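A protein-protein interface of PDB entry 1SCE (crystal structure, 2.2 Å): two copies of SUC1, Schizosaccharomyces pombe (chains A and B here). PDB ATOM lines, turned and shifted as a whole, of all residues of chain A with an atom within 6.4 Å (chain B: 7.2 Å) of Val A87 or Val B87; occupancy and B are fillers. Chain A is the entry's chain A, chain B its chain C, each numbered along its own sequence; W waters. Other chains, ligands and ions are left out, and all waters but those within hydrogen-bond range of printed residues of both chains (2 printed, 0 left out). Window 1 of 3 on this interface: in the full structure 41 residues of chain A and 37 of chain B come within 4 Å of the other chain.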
ATOM      1  N   THR A  60       6.019   4.255  22.042  1.00  0.00           N
ATOM      2  CA  THR A  60       7.275   4.825  21.556  1.00  0.00           C
ATOM      3  C   THR A  60       7.256   6.332  21.384  1.00  0.00           C
ATOM      4  O   THR A  60       8.300   6.976  21.470  1.00  0.00           O
ATOM      5  CB  THR A  60       7.705   4.237  20.183  1.00  0.00           C
ATOM      6  OG1 THR A  60       6.772   4.632  19.163  1.00  0.00           O
ATOM      7  CG2 THR A  60       7.806   2.724  20.242  1.00  0.00           C
ATOM      8  N   TYR A  85       5.599   0.863   7.921  1.00  0.00           N
ATOM      9  CA  TYR A  85       5.900  -0.153   8.923  1.00  0.00           C
ATOM     10  C   TYR A  85       6.541   0.501  10.124  1.00  0.00           C
ATOM     11  O   TYR A  85       6.747   1.715  10.127  1.00  0.00           O
ATOM     12  CB  TYR A  85       6.798  -1.262   8.363  1.00  0.00           C
ATOM     13  CG  TYR A  85       8.144  -0.824   7.859  1.00  0.00           C
ATOM     14  CD1 TYR A  85       8.276  -0.186   6.630  1.00  0.00           C
ATOM     15  CD2 TYR A  85       9.298  -1.092   8.588  1.00  0.00           C
ATOM     16  CE1 TYR A  85       9.527   0.167   6.129  1.00  0.00           C
ATOM     17  CE2 TYR A  85      10.564  -0.734   8.102  1.00  0.00           C
ATOM     18  CZ  TYR A  85      10.668  -0.107   6.870  1.00  0.00           C
ATOM     19  OH  TYR A  85      11.907   0.245   6.384  1.00  0.00           O
ATOM     20  N   GLU A  86       6.847  -0.309  11.136  1.00  0.00           N
ATOM     21  CA  GLU A  86       7.459   0.153  12.379  1.00  0.00           C
ATOM     22  C   GLU A  86       8.576  -0.766  12.877  1.00  0.00           C
ATOM     23  O   GLU A  86       8.704  -1.908  12.448  1.00  0.00           O
ATOM     24  CB  GLU A  86       6.421   0.200  13.487  1.00  0.00           C
ATOM     25  CG  GLU A  86       5.470   1.353  13.454  1.00  0.00           C
ATOM     26  CD  GLU A  86       4.734   1.477  14.769  1.00  0.00           C
ATOM     27  OE1 GLU A  86       4.195   0.447  15.235  1.00  0.00           O
ATOM     28  OE2 GLU A  86       4.731   2.588  15.349  1.00  0.00           O
ATOM     29  N   VAL A  87       9.350  -0.262  13.826  1.00  0.00           N
ATOM     30  CA  VAL A  87      10.429  -1.020  14.433  1.00  0.00           C
ATOM     31  C   VAL A  87       9.986  -1.336  15.859  1.00  0.00           C
ATOM     32  O   VAL A  87       9.658  -0.430  16.634  1.00  0.00           O
ATOM     33  CB  VAL A  87      11.738  -0.207  14.427  1.00  0.00           C
ATOM     34  CG1 VAL A  87      12.833  -0.924  15.212  1.00  0.00           C
ATOM     35  CG2 VAL A  87      12.186   0.006  12.994  1.00  0.00           C
ATOM     36  N   HIS A  88       9.886  -2.623  16.177  1.00  0.00           N
ATOM     37  CA  HIS A  88       9.460  -3.019  17.510  1.00  0.00           C
ATOM     38  C   HIS A  88      10.593  -3.488  18.404  1.00  0.00           C
ATOM     39  O   HIS A  88      11.127  -4.590  18.229  1.00  0.00           O
ATOM     40  CB  HIS A  88       8.373  -4.090  17.466  1.00  0.00           C
ATOM     41  CG  HIS A  88       7.810  -4.411  18.817  1.00  0.00           C
ATOM     42  ND1 HIS A  88       7.576  -5.702  19.245  1.00  0.00           N
ATOM     43  CD2 HIS A  88       7.475  -3.605  19.853  1.00  0.00           C
ATOM     44  CE1 HIS A  88       7.125  -5.677  20.487  1.00  0.00           C
ATOM     45  NE2 HIS A  88       7.054  -4.418  20.879  1.00  0.00           N
ATOM     46  N   VAL A  89      10.916  -2.654  19.389  1.00  0.00           N
ATOM     47  CA  VAL A  89      11.962  -2.939  20.355  1.00  0.00           C
ATOM     48  C   VAL A  89      11.493  -3.973  21.376  1.00  0.00           C
ATOM     49  O   VAL A  89      10.401  -3.864  21.942  1.00  0.00           O
ATOM     50  CB  VAL A  89      12.409  -1.640  21.085  1.00  0.00           C
ATOM     51  CG1 VAL A  89      13.399  -1.954  22.215  1.00  0.00           C
ATOM     52  CG2 VAL A  89      13.077  -0.682  20.088  1.00  0.00           C
ATOM     53  N   PRO A  90      12.287  -5.028  21.582  1.00  0.00           N
ATOM     54  CA  PRO A  90      11.935  -6.074  22.547  1.00  0.00           C
ATOM     55  C   PRO A  90      12.073  -5.604  23.994  1.00  0.00           C
ATOM     56  O   PRO A  90      12.628  -4.534  24.270  1.00  0.00           O
ATOM     57  CB  PRO A  90      12.945  -7.173  22.229  1.00  0.00           C
ATOM     58  CG  PRO A  90      14.131  -6.406  21.748  1.00  0.00           C
ATOM     59  CD  PRO A  90      13.491  -5.402  20.826  1.00  0.00           C
ATOM     60  N   LEU A  96      18.589 -10.357  21.107  1.00  0.00           N
ATOM     61  CA  LEU A  96      18.536 -10.774  19.701  1.00  0.00           C
ATOM     62  C   LEU A  96      19.930 -11.038  19.114  1.00  0.00           C
ATOM     63  O   LEU A  96      20.845 -10.235  19.298  1.00  0.00           O
ATOM     64  CB  LEU A  96      17.820  -9.691  18.869  1.00  0.00           C
ATOM     65  CG  LEU A  96      16.479  -9.094  19.354  1.00  0.00           C
ATOM     66  CD1 LEU A  96      16.098  -7.851  18.515  1.00  0.00           C
ATOM     67  CD2 LEU A  96      15.375 -10.143  19.289  1.00  0.00           C
ATOM     68  N   ILE B  65      24.895  -3.910  23.818  1.00  0.00           N
ATOM     69  CA  ILE B  65      25.476  -4.931  22.953  1.00  0.00           C
ATOM     70  C   ILE B  65      26.615  -5.586  23.727  1.00  0.00           C
ATOM     71  O   ILE B  65      27.434  -4.898  24.335  1.00  0.00           O
ATOM     72  CB  ILE B  65      26.035  -4.321  21.652  1.00  0.00           C
ATOM     73  CG1 ILE B  65      24.902  -3.716  20.834  1.00  0.00           C
ATOM     74  CG2 ILE B  65      26.769  -5.379  20.837  1.00  0.00           C
ATOM     75  CD1 ILE B  65      23.897  -4.725  20.388  1.00  0.00           C
ATOM     76  N   TYR B  85      22.632  -8.326  18.257  1.00  0.00           N
ATOM     77  CA  TYR B  85      22.306  -7.097  17.563  1.00  0.00           C
ATOM     78  C   TYR B  85      21.252  -6.303  18.299  1.00  0.00           C
ATOM     79  O   TYR B  85      20.726  -6.742  19.324  1.00  0.00           O
ATOM     80  CB  TYR B  85      21.934  -7.331  16.096  1.00  0.00           C
ATOM     81  CG  TYR B  85      20.588  -7.943  15.832  1.00  0.00           C
ATOM     82  CD1 TYR B  85      20.431  -9.322  15.805  1.00  0.00           C
ATOM     83  CD2 TYR B  85      19.484  -7.144  15.508  1.00  0.00           C
ATOM     84  CE1 TYR B  85      19.209  -9.906  15.454  1.00  0.00           C
ATOM     85  CE2 TYR B  85      18.259  -7.714  15.152  1.00  0.00           C
ATOM     86  CZ  TYR B  85      18.135  -9.100  15.130  1.00  0.00           C
ATOM     87  OH  TYR B  85      16.945  -9.693  14.800  1.00  0.00           O
ATOM     88  N   GLU B  86      20.948  -5.122  17.781  1.00  0.00           N
ATOM     89  CA  GLU B  86      19.978  -4.256  18.421  1.00  0.00           C
ATOM     90  C   GLU B  86      19.141  -3.558  17.351  1.00  0.00           C
ATOM     91  O   GLU B  86      19.664  -3.252  16.283  1.00  0.00           O
ATOM     92  CB  GLU B  86      20.775  -3.255  19.255  1.00  0.00           C
ATOM     93  CG  GLU B  86      20.028  -2.120  19.884  1.00  0.00           C
ATOM     94  CD  GLU B  86      20.976  -1.174  20.594  1.00  0.00           C
ATOM     95  OE1 GLU B  86      21.728  -0.449  19.902  1.00  0.00           O
ATOM     96  OE2 GLU B  86      20.985  -1.174  21.839  1.00  0.00           O
ATOM     97  N   VAL B  87      17.839  -3.387  17.597  1.00  0.00           N
ATOM     98  CA  VAL B  87      16.966  -2.689  16.645  1.00  0.00           C
ATOM     99  C   VAL B  87      16.895  -1.197  17.016  1.00  0.00           C
ATOM    100  O   VAL B  87      17.007  -0.844  18.196  1.00  0.00           O
ATOM    101  CB  VAL B  87      15.544  -3.291  16.570  1.00  0.00           C
ATOM    102  CG1 VAL B  87      15.595  -4.660  15.963  1.00  0.00           C
ATOM    103  CG2 VAL B  87      14.900  -3.343  17.920  1.00  0.00           C
ATOM    104  N   HIS B  88      16.722  -0.327  16.020  1.00  0.00           N
ATOM    105  CA  HIS B  88      16.687   1.118  16.259  1.00  0.00           C
ATOM    106  C   HIS B  88      15.494   1.860  15.669  1.00  0.00           C
ATOM    107  O   HIS B  88      15.253   1.805  14.467  1.00  0.00           O
ATOM    108  CB  HIS B  88      17.953   1.722  15.697  1.00  0.00           C
ATOM    109  CG  HIS B  88      19.183   0.964  16.063  1.00  0.00           C
ATOM    110  ND1 HIS B  88      19.655  -0.092  15.312  1.00  0.00           N
ATOM    111  CD2 HIS B  88      20.048   1.113  17.095  1.00  0.00           C
ATOM    112  CE1 HIS B  88      20.764  -0.553  15.861  1.00  0.00           C
ATOM    113  NE2 HIS B  88      21.022   0.162  16.944  1.00  0.00           N
ATOM    114  N   VAL B  89      14.784   2.602  16.514  1.00  0.00           N
ATOM    115  CA  VAL B  89      13.607   3.357  16.083  1.00  0.00           C
ATOM    116  C   VAL B  89      14.037   4.759  15.667  1.00  0.00           C
ATOM    117  O   VAL B  89      14.712   5.457  16.428  1.00  0.00           O
ATOM    118  CB  VAL B  89      12.560   3.460  17.233  1.00  0.00           C
ATOM    119  CG1 VAL B  89      11.267   4.132  16.738  1.00  0.00           C
ATOM    120  CG2 VAL B  89      12.247   2.073  17.805  1.00  0.00           C
ATOM    121  N   PRO B  90      13.640   5.198  14.461  1.00  0.00           N
ATOM    122  CA  PRO B  90      14.005   6.536  13.969  1.00  0.00           C
ATOM    123  C   PRO B  90      13.268   7.630  14.750  1.00  0.00           C
ATOM    124  O   PRO B  90      12.346   7.351  15.502  1.00  0.00           O
ATOM    125  CB  PRO B  90      13.556   6.505  12.494  1.00  0.00           C
ATOM    126  CG  PRO B  90      13.431   5.021  12.158  1.00  0.00           C
ATOM    127  CD  PRO B  90      12.894   4.441  13.440  1.00  0.00           C
ATOM    128  N   LEU B  96       8.537   5.332   8.036  1.00  0.00           N
ATOM    129  CA  LEU B  96       9.162   4.324   7.182  1.00  0.00           C
ATOM    130  C   LEU B  96       8.157   3.639   6.261  1.00  0.00           C
ATOM    131  O   LEU B  96       7.052   3.283   6.681  1.00  0.00           O
ATOM    132  CB  LEU B  96       9.872   3.266   8.035  1.00  0.00           C
ATOM    133  CG  LEU B  96      10.923   3.761   9.038  1.00  0.00           C
ATOM    134  CD1 LEU B  96      11.465   2.579   9.881  1.00  0.00           C
ATOM    135  CD2 LEU B  96      12.044   4.497   8.286  1.00  0.00           C
HETATM  136  O   HOH W   1      19.317  -7.589  21.706  1.00  0.00           O
HETATM  137  O   HOH W   2       7.478   4.439  10.431  1.00  0.00           O
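The backbone carbonyl oxygen (O) of Leu B96 is in hydrogen-bond range of the backbone NH (N) of Tyr A85 (3.1 Å).
The backbone carbonyl oxygen (O) of Leu A96 sits at hydrogen-bond distance from the backbone NH (N) of Tyr B85, 2.8 Å away.
A ring nitrogen (NE2) of His B88 lies within hydrogen-bond range of the side-chain carboxylate (OE1) of Glu B86 (3.1 Å).
Among the printed residues, merely in contact across the chains: Val A89 with Val B89, Val A87 with His B88, Val A87 with Val B89, Pro A90 with Val B87, Val A89 with Val B87, Val A87 with Val B87 and His A88 with Val B87.
Of chain B, only Val B87 (3.8 Å), His B88 (3.7 Å) and Val B89 (3.8 Å) come within 4 Å of Val A87.
Printed residues of chain B within 4 Å of His A88: Val B87 (3.99 Å).
Of the printed residues of chain A, His B88 touches Val A87 (3.7 Å).
Printed residues of chain B within 4 Å of Tyr A85: Leu B96.
Pro B90 touches none of the printed residues of chain A.
Of the 8 printed residues of chain B, 5 touch a printed residue of chain A.
Of the 8 printed residues of chain A, 6 touch a printed residue of chain B.
Among the printed residues, no Asp or Glu carboxylate lies within 4 Å of a Lys or Arg side-chain nitrogen of the other chain.
Tyr A85 touches Leu B96, and with the chains exchanged Leu A96 touches Tyr B85.
Val B87 touches its own counterpart, Val A87.
Val A87 touches Val B89, and with the chains exchanged Val A89 touches Val B87.
Val B89 touches its own counterpart, Val A89.
7 positions are printed for both chains.
Water W2 bridges the backbone NH of Leu B96 and the backbone carbonyl oxygen of Tyr A85.
Water W1 lies within hydrogen-bond range of the backbone carbonyl oxygen (O) of Tyr B85 (2.9 Å) and the backbone NH (N) of Leu A96 (2.9 Å).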
